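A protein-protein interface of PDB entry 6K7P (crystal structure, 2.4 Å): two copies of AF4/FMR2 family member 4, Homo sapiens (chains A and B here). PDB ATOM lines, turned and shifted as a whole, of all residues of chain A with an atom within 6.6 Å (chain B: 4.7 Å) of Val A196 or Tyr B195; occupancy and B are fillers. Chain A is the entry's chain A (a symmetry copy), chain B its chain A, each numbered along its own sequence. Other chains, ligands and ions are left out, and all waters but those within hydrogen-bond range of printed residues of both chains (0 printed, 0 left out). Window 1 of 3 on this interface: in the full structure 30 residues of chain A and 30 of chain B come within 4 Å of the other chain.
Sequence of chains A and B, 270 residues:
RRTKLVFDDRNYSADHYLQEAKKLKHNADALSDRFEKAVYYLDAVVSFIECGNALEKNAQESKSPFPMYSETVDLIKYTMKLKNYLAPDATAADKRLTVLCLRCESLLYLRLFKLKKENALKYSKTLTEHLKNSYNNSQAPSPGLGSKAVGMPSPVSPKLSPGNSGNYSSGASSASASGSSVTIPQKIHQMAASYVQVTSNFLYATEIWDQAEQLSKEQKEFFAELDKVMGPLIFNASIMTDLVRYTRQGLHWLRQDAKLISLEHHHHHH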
ATOM      1  N   LEU A 127     -26.144 -10.673  14.677  1.00  0.00           N
ATOM      2  CA  LEU A 127     -27.213  -9.766  15.073  1.00  0.00           C
ATOM      3  C   LEU A 127     -28.570 -10.443  14.990  1.00  0.00           C
ATOM      4  O   LEU A 127     -29.403 -10.284  15.888  1.00  0.00           O
ATOM      5  CB  LEU A 127     -27.200  -8.508  14.212  1.00  0.00           C
ATOM      6  CG  LEU A 127     -26.278  -7.366  14.620  1.00  0.00           C
ATOM      7  CD1 LEU A 127     -26.388  -6.236  13.620  1.00  0.00           C
ATOM      8  CD2 LEU A 127     -26.616  -6.868  16.017  1.00  0.00           C
ATOM      9  N   MET A 191     -22.170  -3.549  17.601  1.00  0.00           N
ATOM     10  CA  MET A 191     -22.301  -4.248  16.333  1.00  0.00           C
ATOM     11  C   MET A 191     -23.557  -3.800  15.591  1.00  0.00           C
ATOM     12  O   MET A 191     -23.559  -3.691  14.359  1.00  0.00           O
ATOM     13  CB  MET A 191     -22.317  -5.749  16.589  1.00  0.00           C
ATOM     14  CG  MET A 191     -22.615  -6.580  15.376  1.00  0.00           C
ATOM     15  SD  MET A 191     -22.408  -8.310  15.774  1.00  0.00           S
ATOM     16  CE  MET A 191     -20.745  -8.306  16.438  1.00  0.00           C
ATOM     17  N   ALA A 192     -24.633  -3.529  16.333  1.00  0.00           N
ATOM     18  CA  ALA A 192     -25.837  -2.971  15.731  1.00  0.00           C
ATOM     19  C   ALA A 192     -25.562  -1.586  15.159  1.00  0.00           C
ATOM     20  O   ALA A 192     -25.959  -1.275  14.022  1.00  0.00           O
ATOM     21  CB  ALA A 192     -26.966  -2.920  16.765  1.00  0.00           C
ATOM     22  N   ALA A 193     -24.867  -0.745  15.933  1.00  0.00           N
ATOM     23  CA  ALA A 193     -24.522   0.585  15.447  1.00  0.00           C
ATOM     24  C   ALA A 193     -23.757   0.509  14.125  1.00  0.00           C
ATOM     25  O   ALA A 193     -24.122   1.169  13.143  1.00  0.00           O
ATOM     26  CB  ALA A 193     -23.712   1.332  16.502  1.00  0.00           C
ATOM     27  N   SER A 194     -22.715  -0.328  14.072  1.00  0.00           N
ATOM     28  CA  SER A 194     -21.875  -0.388  12.872  1.00  0.00           C
ATOM     29  C   SER A 194     -22.609  -1.007  11.695  1.00  0.00           C
ATOM     30  O   SER A 194     -22.456  -0.543  10.561  1.00  0.00           O
ATOM     31  CB  SER A 194     -20.600  -1.172  13.155  1.00  0.00           C
ATOM     32  OG  SER A 194     -19.930  -0.609  14.260  1.00  0.00           O
ATOM     33  N   TYR A 195     -23.379  -2.074  11.934  1.00  0.00           N
ATOM     34  CA  TYR A 195     -24.188  -2.669  10.874  1.00  0.00           C
ATOM     35  C   TYR A 195     -25.089  -1.626  10.222  1.00  0.00           C
ATOM     36  O   TYR A 195     -25.101  -1.480   8.989  1.00  0.00           O
ATOM     37  CB  TYR A 195     -25.023  -3.823  11.427  1.00  0.00           C
ATOM     38  CG  TYR A 195     -25.853  -4.545  10.390  1.00  0.00           C
ATOM     39  CD1 TYR A 195     -25.289  -5.524   9.574  1.00  0.00           C
ATOM     40  CD2 TYR A 195     -27.201  -4.255  10.223  1.00  0.00           C
ATOM     41  CE1 TYR A 195     -26.048  -6.196   8.620  1.00  0.00           C
ATOM     42  CE2 TYR A 195     -27.963  -4.917   9.274  1.00  0.00           C
ATOM     43  CZ  TYR A 195     -27.378  -5.890   8.471  1.00  0.00           C
ATOM     44  OH  TYR A 195     -28.137  -6.555   7.521  1.00  0.00           O
ATOM     45  N   VAL A 196     -25.842  -0.876  11.036  1.00  0.00           N
ATOM     46  CA  VAL A 196     -26.659   0.201  10.477  1.00  0.00           C
ATOM     47  C   VAL A 196     -25.789   1.208   9.721  1.00  0.00           C
ATOM     48  O   VAL A 196     -26.198   1.751   8.684  1.00  0.00           O
ATOM     49  CB  VAL A 196     -27.482   0.872  11.589  1.00  0.00           C
ATOM     50  CG1 VAL A 196     -28.022   2.215  11.137  1.00  0.00           C
ATOM     51  CG2 VAL A 196     -28.621  -0.039  12.012  1.00  0.00           C
ATOM     52  N   GLN A 197     -24.579   1.470  10.227  1.00  0.00           N
ATOM     53  CA  GLN A 197     -23.670   2.411   9.574  1.00  0.00           C
ATOM     54  C   GLN A 197     -23.367   1.992   8.134  1.00  0.00           C
ATOM     55  O   GLN A 197     -23.588   2.755   7.181  1.00  0.00           O
ATOM     56  CB  GLN A 197     -22.376   2.514  10.377  1.00  0.00           C
ATOM     57  CG  GLN A 197     -21.394   3.546   9.866  1.00  0.00           C
ATOM     58  CD  GLN A 197     -21.342   4.739  10.789  1.00  0.00           C
ATOM     59  OE1 GLN A 197     -22.390   5.286  11.167  1.00  0.00           O
ATOM     60  NE2 GLN A 197     -20.133   5.128  11.202  1.00  0.00           N
ATOM     61  N   VAL A 198     -22.858   0.775   7.952  1.00  0.00           N
ATOM     62  CA  VAL A 198     -22.432   0.399   6.610  1.00  0.00           C
ATOM     63  C   VAL A 198     -23.603   0.009   5.709  1.00  0.00           C
ATOM     64  O   VAL A 198     -23.478   0.085   4.478  1.00  0.00           O
ATOM     65  CB  VAL A 198     -21.367  -0.710   6.692  1.00  0.00           C
ATOM     66  CG1 VAL A 198     -20.355  -0.374   7.787  1.00  0.00           C
ATOM     67  CG2 VAL A 198     -22.000  -2.062   6.929  1.00  0.00           C
ATOM     68  N   THR A 199     -24.745  -0.393   6.262  1.00  0.00           N
ATOM     69  CA  THR A 199     -25.892  -0.622   5.392  1.00  0.00           C
ATOM     70  C   THR A 199     -26.535   0.691   4.953  1.00  0.00           C
ATOM     71  O   THR A 199     -27.191   0.761   3.895  1.00  0.00           O
ATOM     72  CB  THR A 199     -26.902  -1.526   6.090  1.00  0.00           C
ATOM     73  OG1 THR A 199     -27.282  -0.945   7.348  1.00  0.00           O
ATOM     74  CG2 THR A 199     -26.267  -2.898   6.309  1.00  0.00           C
ATOM     75  N   SER A 200     -26.345   1.749   5.735  1.00  0.00           N
ATOM     76  CA  SER A 200     -26.884   3.031   5.319  1.00  0.00           C
ATOM     77  C   SER A 200     -26.286   3.456   3.988  1.00  0.00           C
ATOM     78  O   SER A 200     -26.984   4.032   3.143  1.00  0.00           O
ATOM     79  CB  SER A 200     -26.621   4.083   6.392  1.00  0.00           C
ATOM     80  OG  SER A 200     -27.653   5.056   6.380  1.00  0.00           O
ATOM     81  N   ASN A 201     -25.024   3.107   3.763  1.00  0.00           N
ATOM     82  CA  ASN A 201     -24.287   3.612   2.615  1.00  0.00           C
ATOM     83  C   ASN A 201     -24.903   3.151   1.303  1.00  0.00           C
ATOM     84  O   ASN A 201     -25.017   3.940   0.359  1.00  0.00           O
ATOM     85  CB  ASN A 201     -22.838   3.173   2.716  1.00  0.00           C
ATOM     86  CG  ASN A 201     -22.036   4.076   3.608  1.00  0.00           C
ATOM     87  OD1 ASN A 201     -22.285   5.284   3.673  1.00  0.00           O
ATOM     88  ND2 ASN A 201     -21.061   3.503   4.301  1.00  0.00           N
ATOM     89  N   PHE A 202     -25.336   1.898   1.216  1.00  0.00           N
ATOM     90  CA  PHE A 202     -26.001   1.537  -0.018  1.00  0.00           C
ATOM     91  C   PHE A 202     -27.487   1.816  -0.015  1.00  0.00           C
ATOM     92  O   PHE A 202     -28.079   1.809  -1.098  1.00  0.00           O
ATOM     93  CB  PHE A 202     -25.797   0.078  -0.366  1.00  0.00           C
ATOM     94  CG  PHE A 202     -26.015  -0.815   0.753  1.00  0.00           C
ATOM     95  CD1 PHE A 202     -27.241  -0.920   1.316  1.00  0.00           C
ATOM     96  CD2 PHE A 202     -24.988  -1.572   1.239  1.00  0.00           C
ATOM     97  CE1 PHE A 202     -27.423  -1.717   2.373  1.00  0.00           C
ATOM     98  CE2 PHE A 202     -25.168  -2.414   2.286  1.00  0.00           C
ATOM     99  CZ  PHE A 202     -26.388  -2.502   2.842  1.00  0.00           C
ATOM    100  N   LEU A 203     -28.124   2.019   1.154  1.00  0.00           N
ATOM    101  CA  LEU A 203     -29.463   2.601   1.090  1.00  0.00           C
ATOM    102  C   LEU A 203     -29.400   3.942   0.368  1.00  0.00           C
ATOM    103  O   LEU A 203     -30.221   4.244  -0.512  1.00  0.00           O
ATOM    104  CB  LEU A 203     -30.072   2.753   2.494  1.00  0.00           C
ATOM    105  CG  LEU A 203     -30.544   1.445   3.139  1.00  0.00           C
ATOM    106  CD1 LEU A 203     -31.184   1.675   4.518  1.00  0.00           C
ATOM    107  CD2 LEU A 203     -31.496   0.725   2.227  1.00  0.00           C
ATOM    108  N   ALA B 120     -36.678   0.361   5.423  1.00  0.00           N
ATOM    109  CA  ALA B 120     -35.247   0.308   5.704  1.00  0.00           C
ATOM    110  C   ALA B 120     -34.665   1.698   5.891  1.00  0.00           C
ATOM    111  O   ALA B 120     -33.836   1.918   6.782  1.00  0.00           O
ATOM    112  CB  ALA B 120     -34.502  -0.424   4.586  1.00  0.00           C
ATOM    113  N   TYR B 123     -36.085   3.580   9.164  1.00  0.00           N
ATOM    114  CA  TYR B 123     -35.537   2.732  10.220  1.00  0.00           C
ATOM    115  C   TYR B 123     -34.068   3.051  10.438  1.00  0.00           C
ATOM    116  O   TYR B 123     -33.612   3.133  11.583  1.00  0.00           O
ATOM    117  CB  TYR B 123     -35.650   1.234   9.893  1.00  0.00           C
ATOM    118  CG  TYR B 123     -37.008   0.616  10.060  1.00  0.00           C
ATOM    119  CD1 TYR B 123     -38.095   1.347  10.537  1.00  0.00           C
ATOM    120  CD2 TYR B 123     -37.202  -0.718   9.743  1.00  0.00           C
ATOM    121  CE1 TYR B 123     -39.337   0.750  10.685  1.00  0.00           C
ATOM    122  CE2 TYR B 123     -38.435  -1.319   9.882  1.00  0.00           C
ATOM    123  CZ  TYR B 123     -39.500  -0.583  10.354  1.00  0.00           C
ATOM    124  OH  TYR B 123     -40.729  -1.188  10.491  1.00  0.00           O
ATOM    125  N   SER B 124     -33.316   3.202   9.343  1.00  0.00           N
ATOM    126  CA  SER B 124     -31.904   3.556   9.461  1.00  0.00           C
ATOM    127  C   SER B 124     -31.740   4.886  10.176  1.00  0.00           C
ATOM    128  O   SER B 124     -30.863   5.037  11.034  1.00  0.00           O
ATOM    129  CB  SER B 124     -31.250   3.614   8.073  1.00  0.00           C
ATOM    130  OG  SER B 124     -30.219   4.595   8.023  1.00  0.00           O
ATOM    131  N   LEU B 127     -32.850   4.518  13.960  1.00  0.00           N
ATOM    132  CA  LEU B 127     -31.902   3.605  14.586  1.00  0.00           C
ATOM    133  C   LEU B 127     -30.564   4.281  14.831  1.00  0.00           C
ATOM    134  O   LEU B 127     -29.965   4.112  15.897  1.00  0.00           O
ATOM    135  CB  LEU B 127     -31.711   2.357  13.732  1.00  0.00           C
ATOM    136  CG  LEU B 127     -32.701   1.212  13.902  1.00  0.00           C
ATOM    137  CD1 LEU B 127     -32.359   0.092  12.943  1.00  0.00           C
ATOM    138  CD2 LEU B 127     -32.700   0.699  15.333  1.00  0.00           C
ATOM    139  N   THR B 128     -30.070   5.043  13.851  1.00  0.00           N
ATOM    140  CA  THR B 128     -28.802   5.732  14.061  1.00  0.00           C
ATOM    141  C   THR B 128     -28.915   6.715  15.214  1.00  0.00           C
ATOM    142  O   THR B 128     -28.009   6.806  16.052  1.00  0.00           O
ATOM    143  CB  THR B 128     -28.355   6.449  12.788  1.00  0.00           C
ATOM    144  OG1 THR B 128     -28.095   5.486  11.759  1.00  0.00           O
ATOM    145  CG2 THR B 128     -27.080   7.245  13.049  1.00  0.00           C
ATOM    146  N   LEU B 131     -29.297   4.628  18.657  1.00  0.00           N
ATOM    147  CA  LEU B 131     -28.072   3.876  18.929  1.00  0.00           C
ATOM    148  C   LEU B 131     -26.932   4.751  19.295  1.00  0.00           C
ATOM    149  O   LEU B 131     -25.777   4.302  19.391  1.00  0.00           O
ATOM    150  CB  LEU B 131     -27.698   3.030  17.719  1.00  0.00           C
ATOM    151  CG  LEU B 131     -28.553   1.780  17.617  1.00  0.00           C
ATOM    152  CD1 LEU B 131     -28.213   1.006  16.357  1.00  0.00           C
ATOM    153  CD2 LEU B 131     -28.346   0.944  18.867  1.00  0.00           C
ATOM    154  N   MET B 191     -37.389  -2.631  15.795  1.00  0.00           N
ATOM    155  CA  MET B 191     -36.965  -1.920  14.600  1.00  0.00           C
ATOM    156  C   MET B 191     -35.570  -2.362  14.170  1.00  0.00           C
ATOM    157  O   MET B 191     -35.279  -2.457  12.971  1.00  0.00           O
ATOM    158  CB  MET B 191     -37.012  -0.421  14.868  1.00  0.00           C
ATOM    159  CG  MET B 191     -36.439   0.422  13.768  1.00  0.00           C
ATOM    160  SD  MET B 191     -36.735   2.148  14.124  1.00  0.00           S
ATOM    161  CE  MET B 191     -38.508   2.140  14.380  1.00  0.00           C
ATOM    162  N   ALA B 192     -34.698  -2.641  15.140  1.00  0.00           N
ATOM    163  CA  ALA B 192     -33.385  -3.194  14.832  1.00  0.00           C
ATOM    164  C   ALA B 192     -33.517  -4.573  14.197  1.00  0.00           C
ATOM    165  O   ALA B 192     -32.864  -4.873  13.181  1.00  0.00           O
ATOM    166  CB  ALA B 192     -32.531  -3.258  16.101  1.00  0.00           C
ATOM    167  N   ALA B 193     -34.373  -5.421  14.777  1.00  0.00           N
ATOM    168  CA  ALA B 193     -34.593  -6.746  14.209  1.00  0.00           C
ATOM    169  C   ALA B 193     -35.027  -6.655  12.746  1.00  0.00           C
ATOM    170  O   ALA B 193     -34.440  -7.305  11.870  1.00  0.00           O
ATOM    171  CB  ALA B 193     -35.627  -7.502  15.037  1.00  0.00           C
ATOM    172  N   SER B 194     -36.028  -5.816  12.458  1.00  0.00           N
ATOM    173  CA  SER B 194     -36.562  -5.743  11.096  1.00  0.00           C
ATOM    174  C   SER B 194     -35.574  -5.112  10.130  1.00  0.00           C
ATOM    175  O   SER B 194     -35.457  -5.564   8.988  1.00  0.00           O
ATOM    176  CB  SER B 194     -37.869  -4.960  11.080  1.00  0.00           C
ATOM    177  OG  SER B 194     -38.780  -5.533  11.990  1.00  0.00           O
ATOM    178  N   TYR B 195     -34.883  -4.049  10.555  1.00  0.00           N
ATOM    179  CA  TYR B 195     -33.849  -3.443   9.720  1.00  0.00           C
ATOM    180  C   TYR B 195     -32.819  -4.481   9.287  1.00  0.00           C
ATOM    181  O   TYR B 195     -32.517  -4.614   8.090  1.00  0.00           O
ATOM    182  CB  TYR B 195     -33.168  -2.297  10.466  1.00  0.00           C
ATOM    183  CG  TYR B 195     -32.119  -1.564   9.660  1.00  0.00           C
ATOM    184  CD1 TYR B 195     -32.476  -0.577   8.744  1.00  0.00           C
ATOM    185  CD2 TYR B 195     -30.768  -1.855   9.811  1.00  0.00           C
ATOM    186  CE1 TYR B 195     -31.516   0.104   8.002  1.00  0.00           C
ATOM    187  CE2 TYR B 195     -29.806  -1.183   9.074  1.00  0.00           C
ATOM    188  CZ  TYR B 195     -30.187  -0.202   8.167  1.00  0.00           C
ATOM    189  OH  TYR B 195     -29.227   0.472   7.429  1.00  0.00           O
ATOM    190  N   VAL B 196     -32.276  -5.240  10.247  1.00  0.00           N
ATOM    191  CA  VAL B 196     -31.350  -6.312   9.884  1.00  0.00           C
ATOM    192  C   VAL B 196     -32.017  -7.310   8.935  1.00  0.00           C
ATOM    193  O   VAL B 196     -31.375  -7.843   8.017  1.00  0.00           O
ATOM    194  CB  VAL B 196     -30.810  -6.996  11.152  1.00  0.00           C
ATOM    195  CG1 VAL B 196     -30.177  -8.335  10.825  1.00  0.00           C
ATOM    196  CG2 VAL B 196     -29.803  -6.091  11.839  1.00  0.00           C
ATOM    197  N   GLN B 197     -33.311  -7.576   9.140  1.00  0.00           N
ATOM    198  CA  GLN B 197     -34.040  -8.509   8.282  1.00  0.00           C
ATOM    199  C   GLN B 197     -33.998  -8.075   6.816  1.00  0.00           C
ATOM    200  O   GLN B 197     -33.559  -8.828   5.933  1.00  0.00           O
ATOM    201  CB  GLN B 197     -35.487  -8.619   8.758  1.00  0.00           C
ATOM    202  CG  GLN B 197     -36.320  -9.644   8.021  1.00  0.00           C
ATOM    203  CD  GLN B 197     -36.585 -10.847   8.893  1.00  0.00           C
ATOM    204  OE1 GLN B 197     -35.655 -11.399   9.500  1.00  0.00           O
ATOM    205  NE2 GLN B 197     -37.858 -11.239   9.006  1.00  0.00           N
ATOM    206  N   VAL B 198     -34.451  -6.855   6.532  1.00  0.00           N
ATOM    207  CA  VAL B 198     -34.551  -6.464   5.132  1.00  0.00           C
ATOM    208  C   VAL B 198     -33.202  -6.066   4.534  1.00  0.00           C
ATOM    209  O   VAL B 198     -33.034  -6.130   3.308  1.00  0.00           O
ATOM    210  CB  VAL B 198     -35.606  -5.355   4.973  1.00  0.00           C
ATOM    211  CG1 VAL B 198     -36.848  -5.702   5.796  1.00  0.00           C
ATOM    212  CG2 VAL B 198     -35.048  -4.006   5.366  1.00  0.00           C
ATOM    213  N   THR B 199     -32.221  -5.672   5.344  1.00  0.00           N
ATOM    214  CA  THR B 199     -30.903  -5.435   4.770  1.00  0.00           C
ATOM    215  C   THR B 199     -30.173  -6.744   4.480  1.00  0.00           C
ATOM    216  O   THR B 199     -29.287  -6.804   3.606  1.00  0.00           O
ATOM    217  CB  THR B 199     -30.086  -4.540   5.695  1.00  0.00           C
ATOM    218  OG1 THR B 199     -30.011  -5.135   7.002  1.00  0.00           O
ATOM    219  CG2 THR B 199     -30.756  -3.170   5.773  1.00  0.00           C
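OG of Ser B124 lies within hydrogen-bond range of OG of Ser A200. The side-chain hydroxyl of Tyr B195 sits at hydrogen-bond distance from the side-chain hydroxyl of Thr A199 (2.4 Å). OG1 of Thr B199 sits at hydrogen-bond distance from OH of Tyr A195 (2.4 Å).
OG1 of Thr B128 lies within hydrogen-bond range of O of Ser B124 (2.9 Å). The backbone carbonyl oxygen (O) of Tyr B195 lies within hydrogen-bond range of the side-chain hydroxyl (OG1) of Thr B199 (2.8 Å). The backbone carbonyl oxygen (O) of Val B196 is in hydrogen-bond range of the side-chain hydroxyl (OG1) of Thr B199 (3.2 Å). OG1 of Thr A199 is in hydrogen-bond range of O of Tyr A195. OG1 of Thr A199 is in hydrogen-bond range of O of Val A196.
Among the printed residues, merely in contact across the chains: Leu A127 with Val B196, Ala A192 with Leu B131, Ala A193 with Leu B131, Tyr A195 with Val B196, Val A196 with Leu B127, Val A196 with Thr B128, Val A196 with Tyr B195, Ser A200 with Tyr B195, Leu A203 with Ala B120 and Leu A203 with Tyr B195.
Printed residues of chain B within 4 Å of Ala A193: Leu B131 (3.8 Å). Printed residues of chain B within 4 Å of Val A196: Leu B127, Thr B128 and Tyr B195. Of the printed residues of chain A, Ala B120 touches Leu A203 (3.5 Å). Printed residues of chain A within 4 Å of Thr B128: Val A196 (3.3 Å). Met B191 touches none of the printed residues of chain A. Printed residues of chain A within 4 Å of Tyr B195: Val A196 (3.4 Å), Thr A199 (2.4 Å), Ser A200 (3.6 Å) and Leu A203 (3.7 Å). Of the printed residues of chain A, Thr B199 touches Tyr A195. The nearest printed residue of chain B that does not touch Ala A192 is Ala B192 (5.6 Å).
Of the 15 printed residues of chain B, 8 touch a printed residue of chain A. Hydrophobic or aromatic side chains of chain B that line the printed part of chain A: Ala B120, Leu B127, Leu B131, Tyr B195 and Val B196. Printed residues of chain A that touch a printed residue of chain B: Leu A127, Ala A192, Ala A193, Tyr A195, Val A196, Thr A199, Ser A200 and Leu A203. Along chain A the printed residues that touch a printed residue of chain B span positions 127 to 203. Among the printed residues, 13 pairs touch across the chains. Among the printed residues, no Asp or Glu carboxylate lies within 4 Å of a Lys or Arg side-chain nitrogen of the other chain.
Leu A127 touches Val B196, and with the chains exchanged Val A196 touches Leu B127. Tyr A195 touches Val B196, and with the chains exchanged Val A196 touches Tyr B195. Tyr A195 touches Thr B199, and with the chains exchanged Thr A199 touches Tyr B195. 10 positions are printed for both chains.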
